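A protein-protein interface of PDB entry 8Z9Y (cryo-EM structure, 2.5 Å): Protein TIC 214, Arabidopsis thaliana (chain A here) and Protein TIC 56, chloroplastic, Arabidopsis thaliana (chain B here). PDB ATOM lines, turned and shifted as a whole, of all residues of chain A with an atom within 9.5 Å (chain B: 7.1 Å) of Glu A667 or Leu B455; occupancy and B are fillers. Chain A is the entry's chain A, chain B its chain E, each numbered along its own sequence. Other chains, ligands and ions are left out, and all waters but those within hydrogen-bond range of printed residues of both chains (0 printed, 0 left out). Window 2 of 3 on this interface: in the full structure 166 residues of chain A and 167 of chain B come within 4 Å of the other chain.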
ATOM      1  N   VAL A 641      16.416 -24.165  26.790  1.00  0.00           N
ATOM      2  CA  VAL A 641      16.197 -22.807  26.305  1.00  0.00           C
ATOM      3  C   VAL A 641      15.935 -21.865  27.474  1.00  0.00           C
ATOM      4  O   VAL A 641      16.240 -20.668  27.402  1.00  0.00           O
ATOM      5  CB  VAL A 641      15.033 -22.773  25.294  1.00  0.00           C
ATOM      6  CG1 VAL A 641      13.819 -23.505  25.853  1.00  0.00           C
ATOM      7  CG2 VAL A 641      14.677 -21.341  24.925  1.00  0.00           C
ATOM      8  N   VAL A 642      15.407 -22.406  28.574  1.00  0.00           N
ATOM      9  CA  VAL A 642      14.947 -21.564  29.672  1.00  0.00           C
ATOM     10  C   VAL A 642      16.122 -20.816  30.295  1.00  0.00           C
ATOM     11  O   VAL A 642      17.257 -21.311  30.344  1.00  0.00           O
ATOM     12  CB  VAL A 642      14.188 -22.404  30.718  1.00  0.00           C
ATOM     13  CG1 VAL A 642      15.152 -23.166  31.616  1.00  0.00           C
ATOM     14  CG2 VAL A 642      13.265 -21.517  31.544  1.00  0.00           C
ATOM     15  N   PHE A 643      15.850 -19.597  30.752  1.00  0.00           N
ATOM     16  CA  PHE A 643      16.867 -18.753  31.368  1.00  0.00           C
ATOM     17  C   PHE A 643      16.220 -17.654  32.205  1.00  0.00           C
ATOM     18  O   PHE A 643      16.908 -16.805  32.772  1.00  0.00           O
ATOM     19  CB  PHE A 643      17.782 -18.139  30.303  1.00  0.00           C
ATOM     20  CG  PHE A 643      17.220 -16.904  29.652  1.00  0.00           C
ATOM     21  CD1 PHE A 643      16.082 -16.972  28.865  1.00  0.00           C
ATOM     22  CD2 PHE A 643      17.834 -15.675  29.827  1.00  0.00           C
ATOM     23  CE1 PHE A 643      15.567 -15.837  28.266  1.00  0.00           C
ATOM     24  CE2 PHE A 643      17.324 -14.537  29.231  1.00  0.00           C
ATOM     25  CZ  PHE A 643      16.189 -14.618  28.450  1.00  0.00           C
ATOM     26  N   ASP A 666      10.862 -25.118  33.807  1.00  0.00           N
ATOM     27  CA  ASP A 666       9.919 -24.227  34.472  1.00  0.00           C
ATOM     28  C   ASP A 666       8.491 -24.534  34.033  1.00  0.00           C
ATOM     29  O   ASP A 666       7.863 -25.463  34.541  1.00  0.00           O
ATOM     30  CB  ASP A 666      10.267 -22.764  34.183  1.00  0.00           C
ATOM     31  CG  ASP A 666       9.412 -21.793  34.975  1.00  0.00           C
ATOM     32  OD1 ASP A 666       9.716 -21.566  36.165  1.00  0.00           O
ATOM     33  OD2 ASP A 666       8.436 -21.259  34.407  1.00  0.00           O
ATOM     34  N   GLU A 667       7.980 -23.749  33.086  1.00  0.00           N
ATOM     35  CA  GLU A 667       6.634 -23.939  32.561  1.00  0.00           C
ATOM     36  C   GLU A 667       6.631 -24.254  31.073  1.00  0.00           C
ATOM     37  O   GLU A 667       5.987 -25.223  30.654  1.00  0.00           O
ATOM     38  CB  GLU A 667       5.778 -22.694  32.847  1.00  0.00           C
ATOM     39  CG  GLU A 667       4.301 -22.872  32.542  1.00  0.00           C
ATOM     40  CD  GLU A 667       3.487 -23.220  33.772  1.00  0.00           C
ATOM     41  OE1 GLU A 667       3.533 -24.390  34.203  1.00  0.00           O
ATOM     42  OE2 GLU A 667       2.799 -22.325  34.306  1.00  0.00           O
ATOM     43  N   MET A 668       7.329 -23.463  30.262  1.00  0.00           N
ATOM     44  CA  MET A 668       7.474 -23.786  28.849  1.00  0.00           C
ATOM     45  C   MET A 668       8.294 -25.060  28.684  1.00  0.00           C
ATOM     46  O   MET A 668       9.166 -25.374  29.499  1.00  0.00           O
ATOM     47  CB  MET A 668       8.126 -22.624  28.097  1.00  0.00           C
ATOM     48  CG  MET A 668       9.628 -22.506  28.293  1.00  0.00           C
ATOM     49  SD  MET A 668      10.055 -21.733  29.865  1.00  0.00           S
ATOM     50  CE  MET A 668      10.457 -20.073  29.327  1.00  0.00           C
ATOM     51  N   ALA A 669       7.998 -25.811  27.623  1.00  0.00           N
ATOM     52  CA  ALA A 669       8.528 -27.162  27.493  1.00  0.00           C
ATOM     53  C   ALA A 669       9.830 -27.218  26.700  1.00  0.00           C
ATOM     54  O   ALA A 669      10.879 -27.543  27.263  1.00  0.00           O
ATOM     55  CB  ALA A 669       7.471 -28.070  26.849  1.00  0.00           C
ATOM     56  N   LEU A 670       9.795 -26.879  25.411  1.00  0.00           N
ATOM     57  CA  LEU A 670      10.985 -27.015  24.570  1.00  0.00           C
ATOM     58  C   LEU A 670      10.835 -26.158  23.325  1.00  0.00           C
ATOM     59  O   LEU A 670       9.779 -26.178  22.686  1.00  0.00           O
ATOM     60  CB  LEU A 670      11.238 -28.475  24.153  1.00  0.00           C
ATOM     61  CG  LEU A 670      11.384 -29.705  25.057  1.00  0.00           C
ATOM     62  CD1 LEU A 670      10.055 -30.236  25.584  1.00  0.00           C
ATOM     63  CD2 LEU A 670      12.123 -30.781  24.312  1.00  0.00           C
ATOM     64  N   ILE A 671      11.889 -25.418  22.979  1.00  0.00           N
ATOM     65  CA  ILE A 671      12.097 -24.863  21.646  1.00  0.00           C
ATOM     66  C   ILE A 671      13.558 -25.093  21.267  1.00  0.00           C
ATOM     67  O   ILE A 671      14.317 -25.721  22.010  1.00  0.00           O
ATOM     68  CB  ILE A 671      11.718 -23.369  21.550  1.00  0.00           C
ATOM     69  CG1 ILE A 671      12.723 -22.497  22.295  1.00  0.00           C
ATOM     70  CG2 ILE A 671      10.302 -23.118  22.060  1.00  0.00           C
ATOM     71  CD1 ILE A 671      12.745 -21.067  21.811  1.00  0.00           C
ATOM     72  N   ARG B 450       2.486 -24.922  19.818  1.00  0.00           N
ATOM     73  CA  ARG B 450       2.110 -25.699  20.996  1.00  0.00           C
ATOM     74  C   ARG B 450       2.539 -24.996  22.275  1.00  0.00           C
ATOM     75  O   ARG B 450       1.821 -25.028  23.280  1.00  0.00           O
ATOM     76  CB  ARG B 450       2.713 -27.101  20.925  1.00  0.00           C
ATOM     77  CG  ARG B 450       1.996 -28.041  19.974  1.00  0.00           C
ATOM     78  CD  ARG B 450       2.497 -29.465  20.137  1.00  0.00           C
ATOM     79  NE  ARG B 450       2.029 -30.337  19.066  1.00  0.00           N
ATOM     80  CZ  ARG B 450       2.758 -30.693  18.018  1.00  0.00           C
ATOM     81  NH1 ARG B 450       4.002 -30.270  17.865  1.00  0.00           N
ATOM     82  NH2 ARG B 450       2.226 -31.495  17.100  1.00  0.00           N
ATOM     83  N   ILE B 451       3.716 -24.366  22.261  1.00  0.00           N
ATOM     84  CA  ILE B 451       4.145 -23.589  23.421  1.00  0.00           C
ATOM     85  C   ILE B 451       3.165 -22.452  23.690  1.00  0.00           C
ATOM     86  O   ILE B 451       2.759 -22.221  24.835  1.00  0.00           O
ATOM     87  CB  ILE B 451       5.579 -23.064  23.217  1.00  0.00           C
ATOM     88  CG1 ILE B 451       6.576 -24.223  23.173  1.00  0.00           C
ATOM     89  CG2 ILE B 451       5.952 -22.087  24.321  1.00  0.00           C
ATOM     90  CD1 ILE B 451       6.349 -25.270  24.239  1.00  0.00           C
ATOM     91  N   PHE B 452       2.764 -21.733  22.640  1.00  0.00           N
ATOM     92  CA  PHE B 452       1.896 -20.570  22.815  1.00  0.00           C
ATOM     93  C   PHE B 452       0.517 -21.007  23.311  1.00  0.00           C
ATOM     94  O   PHE B 452      -0.012 -20.446  24.276  1.00  0.00           O
ATOM     95  CB  PHE B 452       1.817 -19.807  21.479  1.00  0.00           C
ATOM     96  CG  PHE B 452       1.010 -18.504  21.496  1.00  0.00           C
ATOM     97  CD1 PHE B 452       0.068 -18.203  22.469  1.00  0.00           C
ATOM     98  CD2 PHE B 452       1.225 -17.570  20.494  1.00  0.00           C
ATOM     99  CE1 PHE B 452      -0.636 -17.011  22.440  1.00  0.00           C
ATOM    100  CE2 PHE B 452       0.526 -16.377  20.461  1.00  0.00           C
ATOM    101  CZ  PHE B 452      -0.406 -16.098  21.435  1.00  0.00           C
ATOM    102  N   TYR B 453      -0.058 -22.040  22.691  1.00  0.00           N
ATOM    103  CA  TYR B 453      -1.456 -22.378  22.941  1.00  0.00           C
ATOM    104  C   TYR B 453      -1.708 -22.758  24.396  1.00  0.00           C
ATOM    105  O   TYR B 453      -2.805 -22.525  24.915  1.00  0.00           O
ATOM    106  CB  TYR B 453      -1.888 -23.510  22.008  1.00  0.00           C
ATOM    107  CG  TYR B 453      -3.016 -24.361  22.542  1.00  0.00           C
ATOM    108  CD1 TYR B 453      -4.331 -23.920  22.475  1.00  0.00           C
ATOM    109  CD2 TYR B 453      -2.771 -25.605  23.106  1.00  0.00           C
ATOM    110  CE1 TYR B 453      -5.369 -24.690  22.959  1.00  0.00           C
ATOM    111  CE2 TYR B 453      -3.801 -26.381  23.595  1.00  0.00           C
ATOM    112  CZ  TYR B 453      -5.099 -25.920  23.517  1.00  0.00           C
ATOM    113  OH  TYR B 453      -6.133 -26.689  23.999  1.00  0.00           O
ATOM    114  N   ASN B 454      -0.714 -23.332  25.072  1.00  0.00           N
ATOM    115  CA  ASN B 454      -0.904 -23.795  26.441  1.00  0.00           C
ATOM    116  C   ASN B 454      -0.708 -22.684  27.469  1.00  0.00           C
ATOM    117  O   ASN B 454      -1.486 -22.576  28.422  1.00  0.00           O
ATOM    118  CB  ASN B 454       0.044 -24.960  26.737  1.00  0.00           C
ATOM    119  CG  ASN B 454      -0.571 -25.986  27.670  1.00  0.00           C
ATOM    120  OD1 ASN B 454      -0.605 -25.794  28.885  1.00  0.00           O
ATOM    121  ND2 ASN B 454      -1.061 -27.082  27.104  1.00  0.00           N
ATOM    122  N   LEU B 455       0.319 -21.855  27.296  1.00  0.00           N
ATOM    123  CA  LEU B 455       0.677 -20.836  28.273  1.00  0.00           C
ATOM    124  C   LEU B 455       0.777 -19.470  27.609  1.00  0.00           C
ATOM    125  O   LEU B 455       1.105 -19.370  26.423  1.00  0.00           O
ATOM    126  CB  LEU B 455       1.997 -21.199  28.975  1.00  0.00           C
ATOM    127  CG  LEU B 455       3.217 -21.662  28.164  1.00  0.00           C
ATOM    128  CD1 LEU B 455       3.858 -20.558  27.327  1.00  0.00           C
ATOM    129  CD2 LEU B 455       4.243 -22.297  29.076  1.00  0.00           C
ATOM    130  N   SER B 456       0.495 -18.425  28.383  1.00  0.00           N
ATOM    131  CA  SER B 456       0.552 -17.045  27.901  1.00  0.00           C
ATOM    132  C   SER B 456      -0.345 -16.833  26.684  1.00  0.00           C
ATOM    133  O   SER B 456      -1.569 -16.776  26.805  1.00  0.00           O
ATOM    134  CB  SER B 456       1.993 -16.651  27.565  1.00  0.00           C
ATOM    135  OG  SER B 456       2.033 -15.448  26.817  1.00  0.00           O
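Glu A667 touches Leu B455 (CG to CD2, 3.5 Å). Met A668 touches Leu B455. CD1 of Ile B451 touches N of Ala A669, at 3.8 Å. Ile B451 touches Leu A670.
Glu A667 touches just one residue of chain B: Leu B455 (3.5 Å). No residue of chain A comes within 4 Å of Ser B456. Of the printed residues of chain B, Ala A669 touches Ile B451 (3.8 Å). Of the printed residues of chain B, Met A668 touches Leu B455. Of the printed residues of chain A, Ile B451 touches Ala A669 (3.8 Å) and Leu A670 (3.8 Å). Of the printed residues of chain B, Leu A670 touches Ile B451 (3.8 Å). The nearest residue of chain B that does not touch Glu A667 is Ile B451 (6.4 Å). The nearest residue of chain A that does not touch Leu B455 is Ala A669 (5.3 Å). The nearest printed residue of chain B that does not touch Leu A670 is Arg B450 (7.3 Å).
Of the 7 printed residues of chain B, 2 touch a printed residue of chain A. Of the 9 printed residues of chain A, 4 touch a printed residue of chain B. Hydrophobic or aromatic side chains of chain A that line the printed part of chain B: Ala A669. Along chain A the printed residues that touch a printed residue of chain B span positions 667 to 670. Among the printed residues, no Asp or Glu carboxylate lies within 4 Å of a Lys or Arg side-chain nitrogen of the other chain.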
